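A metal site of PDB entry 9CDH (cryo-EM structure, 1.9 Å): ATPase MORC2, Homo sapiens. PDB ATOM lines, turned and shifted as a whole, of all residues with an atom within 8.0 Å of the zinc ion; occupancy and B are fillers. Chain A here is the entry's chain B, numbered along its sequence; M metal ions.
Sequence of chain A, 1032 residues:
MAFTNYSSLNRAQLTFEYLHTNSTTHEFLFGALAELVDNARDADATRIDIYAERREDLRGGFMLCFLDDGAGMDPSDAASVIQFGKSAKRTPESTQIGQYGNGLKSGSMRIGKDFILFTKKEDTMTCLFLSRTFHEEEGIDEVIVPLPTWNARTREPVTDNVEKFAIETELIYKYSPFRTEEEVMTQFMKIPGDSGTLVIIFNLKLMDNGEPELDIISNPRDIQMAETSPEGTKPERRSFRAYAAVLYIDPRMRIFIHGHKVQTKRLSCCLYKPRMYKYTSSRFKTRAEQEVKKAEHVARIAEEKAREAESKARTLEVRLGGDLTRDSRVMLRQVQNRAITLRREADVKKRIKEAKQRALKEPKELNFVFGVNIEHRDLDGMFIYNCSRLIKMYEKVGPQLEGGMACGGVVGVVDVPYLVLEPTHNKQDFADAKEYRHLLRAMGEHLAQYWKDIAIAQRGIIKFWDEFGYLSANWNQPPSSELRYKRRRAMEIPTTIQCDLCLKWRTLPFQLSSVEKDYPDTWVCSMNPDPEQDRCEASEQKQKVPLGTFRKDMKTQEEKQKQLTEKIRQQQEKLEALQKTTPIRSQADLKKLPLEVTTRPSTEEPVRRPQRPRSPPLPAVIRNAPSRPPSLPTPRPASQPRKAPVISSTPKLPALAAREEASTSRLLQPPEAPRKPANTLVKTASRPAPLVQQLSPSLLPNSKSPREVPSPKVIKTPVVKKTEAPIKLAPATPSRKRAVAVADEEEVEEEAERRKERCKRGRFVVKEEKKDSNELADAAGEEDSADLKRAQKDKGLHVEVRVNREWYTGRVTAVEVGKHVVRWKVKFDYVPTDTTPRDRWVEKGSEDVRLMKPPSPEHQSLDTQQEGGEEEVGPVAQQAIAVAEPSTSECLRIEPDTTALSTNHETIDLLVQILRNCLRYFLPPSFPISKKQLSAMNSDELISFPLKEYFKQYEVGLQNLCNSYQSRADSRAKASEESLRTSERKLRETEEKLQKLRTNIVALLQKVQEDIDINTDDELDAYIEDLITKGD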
ATOM      1  N   GLN A 498      11.166  19.310 -33.728  1.00  0.00           N
ATOM      2  CA  GLN A 498      10.596  19.267 -32.390  1.00  0.00           C
ATOM      3  C   GLN A 498      10.542  17.822 -31.911  1.00  0.00           C
ATOM      4  O   GLN A 498      10.075  16.940 -32.635  1.00  0.00           O
ATOM      5  CB  GLN A 498       9.200  19.874 -32.368  1.00  0.00           C
ATOM      6  CG  GLN A 498       8.730  20.322 -30.990  1.00  0.00           C
ATOM      7  CD  GLN A 498       7.219  20.248 -30.829  1.00  0.00           C
ATOM      8  OE1 GLN A 498       6.499  20.090 -31.807  1.00  0.00           O
ATOM      9  NE2 GLN A 498       6.743  20.385 -29.599  1.00  0.00           N
ATOM     10  N   CYS A 499      11.016  17.585 -30.694  1.00  0.00           N
ATOM     11  CA  CYS A 499      10.965  16.258 -30.113  1.00  0.00           C
ATOM     12  C   CYS A 499       9.527  15.862 -29.795  1.00  0.00           C
ATOM     13  O   CYS A 499       8.731  16.694 -29.347  1.00  0.00           O
ATOM     14  CB  CYS A 499      11.817  16.201 -28.836  1.00  0.00           C
ATOM     15  SG  CYS A 499      11.596  14.685 -27.884  1.00  0.00           S
ATOM     16  N   ASP A 500       9.207  14.606 -30.049  1.00  0.00           N
ATOM     17  CA  ASP A 500       7.864  14.087 -29.786  1.00  0.00           C
ATOM     18  C   ASP A 500       7.658  13.694 -28.335  1.00  0.00           C
ATOM     19  O   ASP A 500       6.525  13.359 -27.960  1.00  0.00           O
ATOM     20  CB  ASP A 500       7.588  12.878 -30.692  1.00  0.00           C
ATOM     21  CG  ASP A 500       6.105  12.636 -30.896  1.00  0.00           C
ATOM     22  OD1 ASP A 500       5.292  13.475 -30.472  1.00  0.00           O
ATOM     23  OD2 ASP A 500       5.756  11.596 -31.497  1.00  0.00           O
ATOM     24  N   LEU A 501       8.706  13.723 -27.506  1.00  0.00           N
ATOM     25  CA  LEU A 501       8.617  13.284 -26.121  1.00  0.00           C
ATOM     26  C   LEU A 501       8.666  14.417 -25.114  1.00  0.00           C
ATOM     27  O   LEU A 501       7.988  14.338 -24.091  1.00  0.00           O
ATOM     28  CB  LEU A 501       9.754  12.299 -25.807  1.00  0.00           C
ATOM     29  CG  LEU A 501       9.575  11.361 -24.613  1.00  0.00           C
ATOM     30  CD1 LEU A 501       8.235  10.635 -24.654  1.00  0.00           C
ATOM     31  CD2 LEU A 501      10.717  10.365 -24.543  1.00  0.00           C
ATOM     32  N   CYS A 502       9.451  15.467 -25.380  1.00  0.00           N
ATOM     33  CA  CYS A 502       9.554  16.600 -24.473  1.00  0.00           C
ATOM     34  C   CYS A 502       9.121  17.917 -25.093  1.00  0.00           C
ATOM     35  O   CYS A 502       9.080  18.929 -24.386  1.00  0.00           O
ATOM     36  CB  CYS A 502      10.984  16.750 -23.948  1.00  0.00           C
ATOM     37  SG  CYS A 502      12.195  17.196 -25.204  1.00  0.00           S
ATOM     38  N   LEU A 503       8.818  17.938 -26.398  1.00  0.00           N
ATOM     39  CA  LEU A 503       8.291  19.097 -27.112  1.00  0.00           C
ATOM     40  C   LEU A 503       9.341  20.163 -27.375  1.00  0.00           C
ATOM     41  O   LEU A 503       8.993  21.251 -27.855  1.00  0.00           O
ATOM     42  CB  LEU A 503       7.113  19.733 -26.355  1.00  0.00           C
ATOM     43  CG  LEU A 503       5.955  18.805 -25.991  1.00  0.00           C
ATOM     44  CD1 LEU A 503       4.863  19.564 -25.248  1.00  0.00           C
ATOM     45  CD2 LEU A 503       5.383  18.127 -27.228  1.00  0.00           C
ATOM     46  N   LYS A 504      10.618  19.894 -27.091  1.00  0.00           N
ATOM     47  CA  LYS A 504      11.650  20.886 -27.300  1.00  0.00           C
ATOM     48  C   LYS A 504      12.108  20.879 -28.752  1.00  0.00           C
ATOM     49  O   LYS A 504      12.056  19.854 -29.443  1.00  0.00           O
ATOM     50  CB  LYS A 504      12.843  20.613 -26.383  1.00  0.00           C
ATOM     51  CG  LYS A 504      12.876  21.471 -25.132  1.00  0.00           C
ATOM     52  CD  LYS A 504      14.192  21.343 -24.387  1.00  0.00           C
ATOM     53  CE  LYS A 504      14.249  20.080 -23.535  1.00  0.00           C
ATOM     54  NZ  LYS A 504      13.151  19.989 -22.541  1.00  0.00           N
ATOM     55  N   TRP A 505      12.568  22.040 -29.222  1.00  0.00           N
ATOM     56  CA  TRP A 505      12.970  22.226 -30.608  1.00  0.00           C
ATOM     57  C   TRP A 505      14.481  22.147 -30.723  1.00  0.00           C
ATOM     58  O   TRP A 505      15.196  22.761 -29.926  1.00  0.00           O
ATOM     59  CB  TRP A 505      12.466  23.564 -31.147  1.00  0.00           C
ATOM     60  CG  TRP A 505      10.994  23.581 -31.409  1.00  0.00           C
ATOM     61  CD1 TRP A 505      10.011  23.913 -30.526  1.00  0.00           C
ATOM     62  CD2 TRP A 505      10.339  23.228 -32.628  1.00  0.00           C
ATOM     63  NE1 TRP A 505       8.785  23.792 -31.119  1.00  0.00           N
ATOM     64  CE2 TRP A 505       8.958  23.377 -32.417  1.00  0.00           C
ATOM     65  CE3 TRP A 505      10.783  22.805 -33.889  1.00  0.00           C
ATOM     66  CZ2 TRP A 505       8.014  23.115 -33.405  1.00  0.00           C
ATOM     67  CZ3 TRP A 505       9.844  22.549 -34.870  1.00  0.00           C
ATOM     68  CH2 TRP A 505       8.474  22.703 -34.624  1.00  0.00           C
ATOM     69  N   ARG A 506      14.966  21.398 -31.711  1.00  0.00           N
ATOM     70  CA  ARG A 506      16.388  21.221 -31.950  1.00  0.00           C
ATOM     71  C   ARG A 506      16.693  21.493 -33.411  1.00  0.00           C
ATOM     72  O   ARG A 506      15.850  21.283 -34.292  1.00  0.00           O
ATOM     73  CB  ARG A 506      16.868  19.806 -31.581  1.00  0.00           C
ATOM     74  CG  ARG A 506      16.144  19.176 -30.406  1.00  0.00           C
ATOM     75  CD  ARG A 506      16.547  19.828 -29.086  1.00  0.00           C
ATOM     76  NE  ARG A 506      16.276  18.963 -27.942  1.00  0.00           N
ATOM     77  CZ  ARG A 506      16.660  19.222 -26.713  1.00  0.00           C
ATOM     78  NH1 ARG A 506      17.356  20.308 -26.414  1.00  0.00           N
ATOM     79  NH2 ARG A 506      16.353  18.360 -25.738  1.00  0.00           N
ATOM     80  N   TRP A 523       9.980  11.908 -33.996  1.00  0.00           N
ATOM     81  CA  TRP A 523      11.399  12.168 -33.784  1.00  0.00           C
ATOM     82  C   TRP A 523      11.627  12.609 -32.350  1.00  0.00           C
ATOM     83  O   TRP A 523      10.840  13.409 -31.813  1.00  0.00           O
ATOM     84  CB  TRP A 523      11.907  13.226 -34.766  1.00  0.00           C
ATOM     85  CG  TRP A 523      13.388  13.455 -34.697  1.00  0.00           C
ATOM     86  CD1 TRP A 523      14.342  12.929 -35.517  1.00  0.00           C
ATOM     87  CD2 TRP A 523      14.081  14.283 -33.750  1.00  0.00           C
ATOM     88  NE1 TRP A 523      15.583  13.369 -35.143  1.00  0.00           N
ATOM     89  CE2 TRP A 523      15.447  14.198 -34.057  1.00  0.00           C
ATOM     90  CE3 TRP A 523      13.674  15.075 -32.676  1.00  0.00           C
ATOM     91  CZ2 TRP A 523      16.418  14.889 -33.338  1.00  0.00           C
ATOM     92  CZ3 TRP A 523      14.634  15.758 -31.955  1.00  0.00           C
ATOM     93  CH2 TRP A 523      15.989  15.658 -32.288  1.00  0.00           C
ATOM     94  N   VAL A 524      12.689  12.113 -31.715  1.00  0.00           N
ATOM     95  CA  VAL A 524      13.017  12.471 -30.345  1.00  0.00           C
ATOM     96  C   VAL A 524      14.468  12.929 -30.284  1.00  0.00           C
ATOM     97  O   VAL A 524      15.226  12.789 -31.258  1.00  0.00           O
ATOM     98  CB  VAL A 524      12.781  11.297 -29.356  1.00  0.00           C
ATOM     99  CG1 VAL A 524      11.304  10.949 -29.314  1.00  0.00           C
ATOM    100  CG2 VAL A 524      13.607  10.082 -29.750  1.00  0.00           C
ATOM    101  N   CYS A 525      14.852  13.483 -29.137  1.00  0.00           N
ATOM    102  CA  CYS A 525      16.184  14.055 -28.991  1.00  0.00           C
ATOM    103  C   CYS A 525      17.282  13.013 -29.203  1.00  0.00           C
ATOM    104  O   CYS A 525      18.376  13.352 -29.647  1.00  0.00           O
ATOM    105  CB  CYS A 525      16.325  14.696 -27.617  1.00  0.00           C
ATOM    106  SG  CYS A 525      15.148  16.035 -27.314  1.00  0.00           S
ATOM    107  N   SER A 526      17.000  11.750 -28.885  1.00  0.00           N
ATOM    108  CA  SER A 526      17.993  10.704 -29.063  1.00  0.00           C
ATOM    109  C   SER A 526      18.336  10.494 -30.533  1.00  0.00           C
ATOM    110  O   SER A 526      19.467  10.141 -30.867  1.00  0.00           O
ATOM    111  CB  SER A 526      17.501   9.392 -28.454  1.00  0.00           C
ATOM    112  OG  SER A 526      17.310   9.529 -27.056  1.00  0.00           O
ATOM    113  N   ASP A 534      23.133  14.852 -27.376  1.00  0.00           N
ATOM    114  CA  ASP A 534      21.821  15.484 -27.256  1.00  0.00           C
ATOM    115  C   ASP A 534      20.830  14.528 -26.604  1.00  0.00           C
ATOM    116  O   ASP A 534      20.838  13.332 -26.871  1.00  0.00           O
ATOM    117  CB  ASP A 534      21.320  15.939 -28.624  1.00  0.00           C
ATOM    118  CG  ASP A 534      20.031  16.719 -28.533  1.00  0.00           C
ATOM    119  OD1 ASP A 534      20.076  17.894 -28.113  1.00  0.00           O
ATOM    120  OD2 ASP A 534      18.963  16.168 -28.896  1.00  0.00           O
ATOM    121  N   ARG A 535      19.956  15.080 -25.766  1.00  0.00           N
ATOM    122  CA  ARG A 535      18.974  14.274 -25.049  1.00  0.00           C
ATOM    123  C   ARG A 535      17.809  15.163 -24.662  1.00  0.00           C
ATOM    124  O   ARG A 535      17.857  16.389 -24.809  1.00  0.00           O
ATOM    125  CB  ARG A 535      19.584  13.595 -23.819  1.00  0.00           C
ATOM    126  CG  ARG A 535      20.112  14.570 -22.774  1.00  0.00           C
ATOM    127  CD  ARG A 535      20.787  13.841 -21.625  1.00  0.00           C
ATOM    128  NE  ARG A 535      21.992  13.148 -22.054  1.00  0.00           N
ATOM    129  CZ  ARG A 535      23.177  13.728 -22.227  1.00  0.00           C
ATOM    130  NH1 ARG A 535      23.347  15.029 -22.010  1.00  0.00           N
ATOM    131  NH2 ARG A 535      24.213  12.986 -22.619  1.00  0.00           N
ATOM    132  N   CYS A 536      16.744  14.533 -24.152  1.00  0.00           N
ATOM    133  CA  CYS A 536      15.558  15.277 -23.772  1.00  0.00           C
ATOM    134  C   CYS A 536      15.829  16.252 -22.639  1.00  0.00           C
ATOM    135  O   CYS A 536      15.132  17.263 -22.503  1.00  0.00           O
ATOM    136  CB  CYS A 536      14.439  14.301 -23.365  1.00  0.00           C
ATOM    137  SG  CYS A 536      13.478  13.676 -24.758  1.00  0.00           S
ATOM    138  N   GLU A 537      16.839  15.983 -21.823  1.00  0.00           N
ATOM    139  CA  GLU A 537      17.187  16.846 -20.703  1.00  0.00           C
ATOM    140  C   GLU A 537      18.079  18.014 -21.098  1.00  0.00           C
ATOM    141  O   GLU A 537      18.318  18.898 -20.264  1.00  0.00           O
ATOM    142  CB  GLU A 537      17.882  16.028 -19.604  1.00  0.00           C
ATOM    143  CG  GLU A 537      16.926  15.188 -18.761  1.00  0.00           C
ATOM    144  CD  GLU A 537      16.311  14.042 -19.546  1.00  0.00           C
ATOM    145  OE1 GLU A 537      16.625  13.896 -20.748  1.00  0.00           O
ATOM    146  OE2 GLU A 537      15.511  13.284 -18.960  1.00  0.00           O
ATOM    147  N   ALA A 538      18.565  18.048 -22.334  1.00  0.00           N
ATOM    148  CA  ALA A 538      19.412  19.143 -22.785  1.00  0.00           C
ATOM    149  C   ALA A 538      18.566  20.393 -23.005  1.00  0.00           C
ATOM    150  O   ALA A 538      17.447  20.333 -23.522  1.00  0.00           O
ATOM    151  CB  ALA A 538      20.127  18.771 -24.080  1.00  0.00           C
HETATM  152 ZN    ZN M   1      13.153  15.391 -26.307  1.00  0.00          ZN
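SG of Cys 502 lies close to N of Lys 504 (3.7 Å).
The side-chain sulfur (SG) of Cys 499 sits close to the backbone NH (N) of Leu 501 (3.1 Å).
N of Cys 499 lies within hydrogen-bond range of O of Lys 504.
SG of Cys 525 lies close to NH2 of Arg 506 (3.1 Å).
The side-chain sulfur (SG) of Cys 525 sits close to the backbone carbonyl oxygen (O) of Arg 535, 3.7 Å away.
The backbone carbonyl oxygen of Cys 536 lies close to the side-chain amino group of Lys 504.
The nearest printed residue that does not touch the zinc ion is Arg 506 (4.4 Å).
The zinc ion is bound by the side-chain sulfur of Cys 502 (2.3 Å), the side-chain sulfur of Cys 499 (2.3 Å), the side-chain sulfur of Cys 525 (2.3 Å) and the side-chain sulfur of Cys 536 (2.3 Å).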
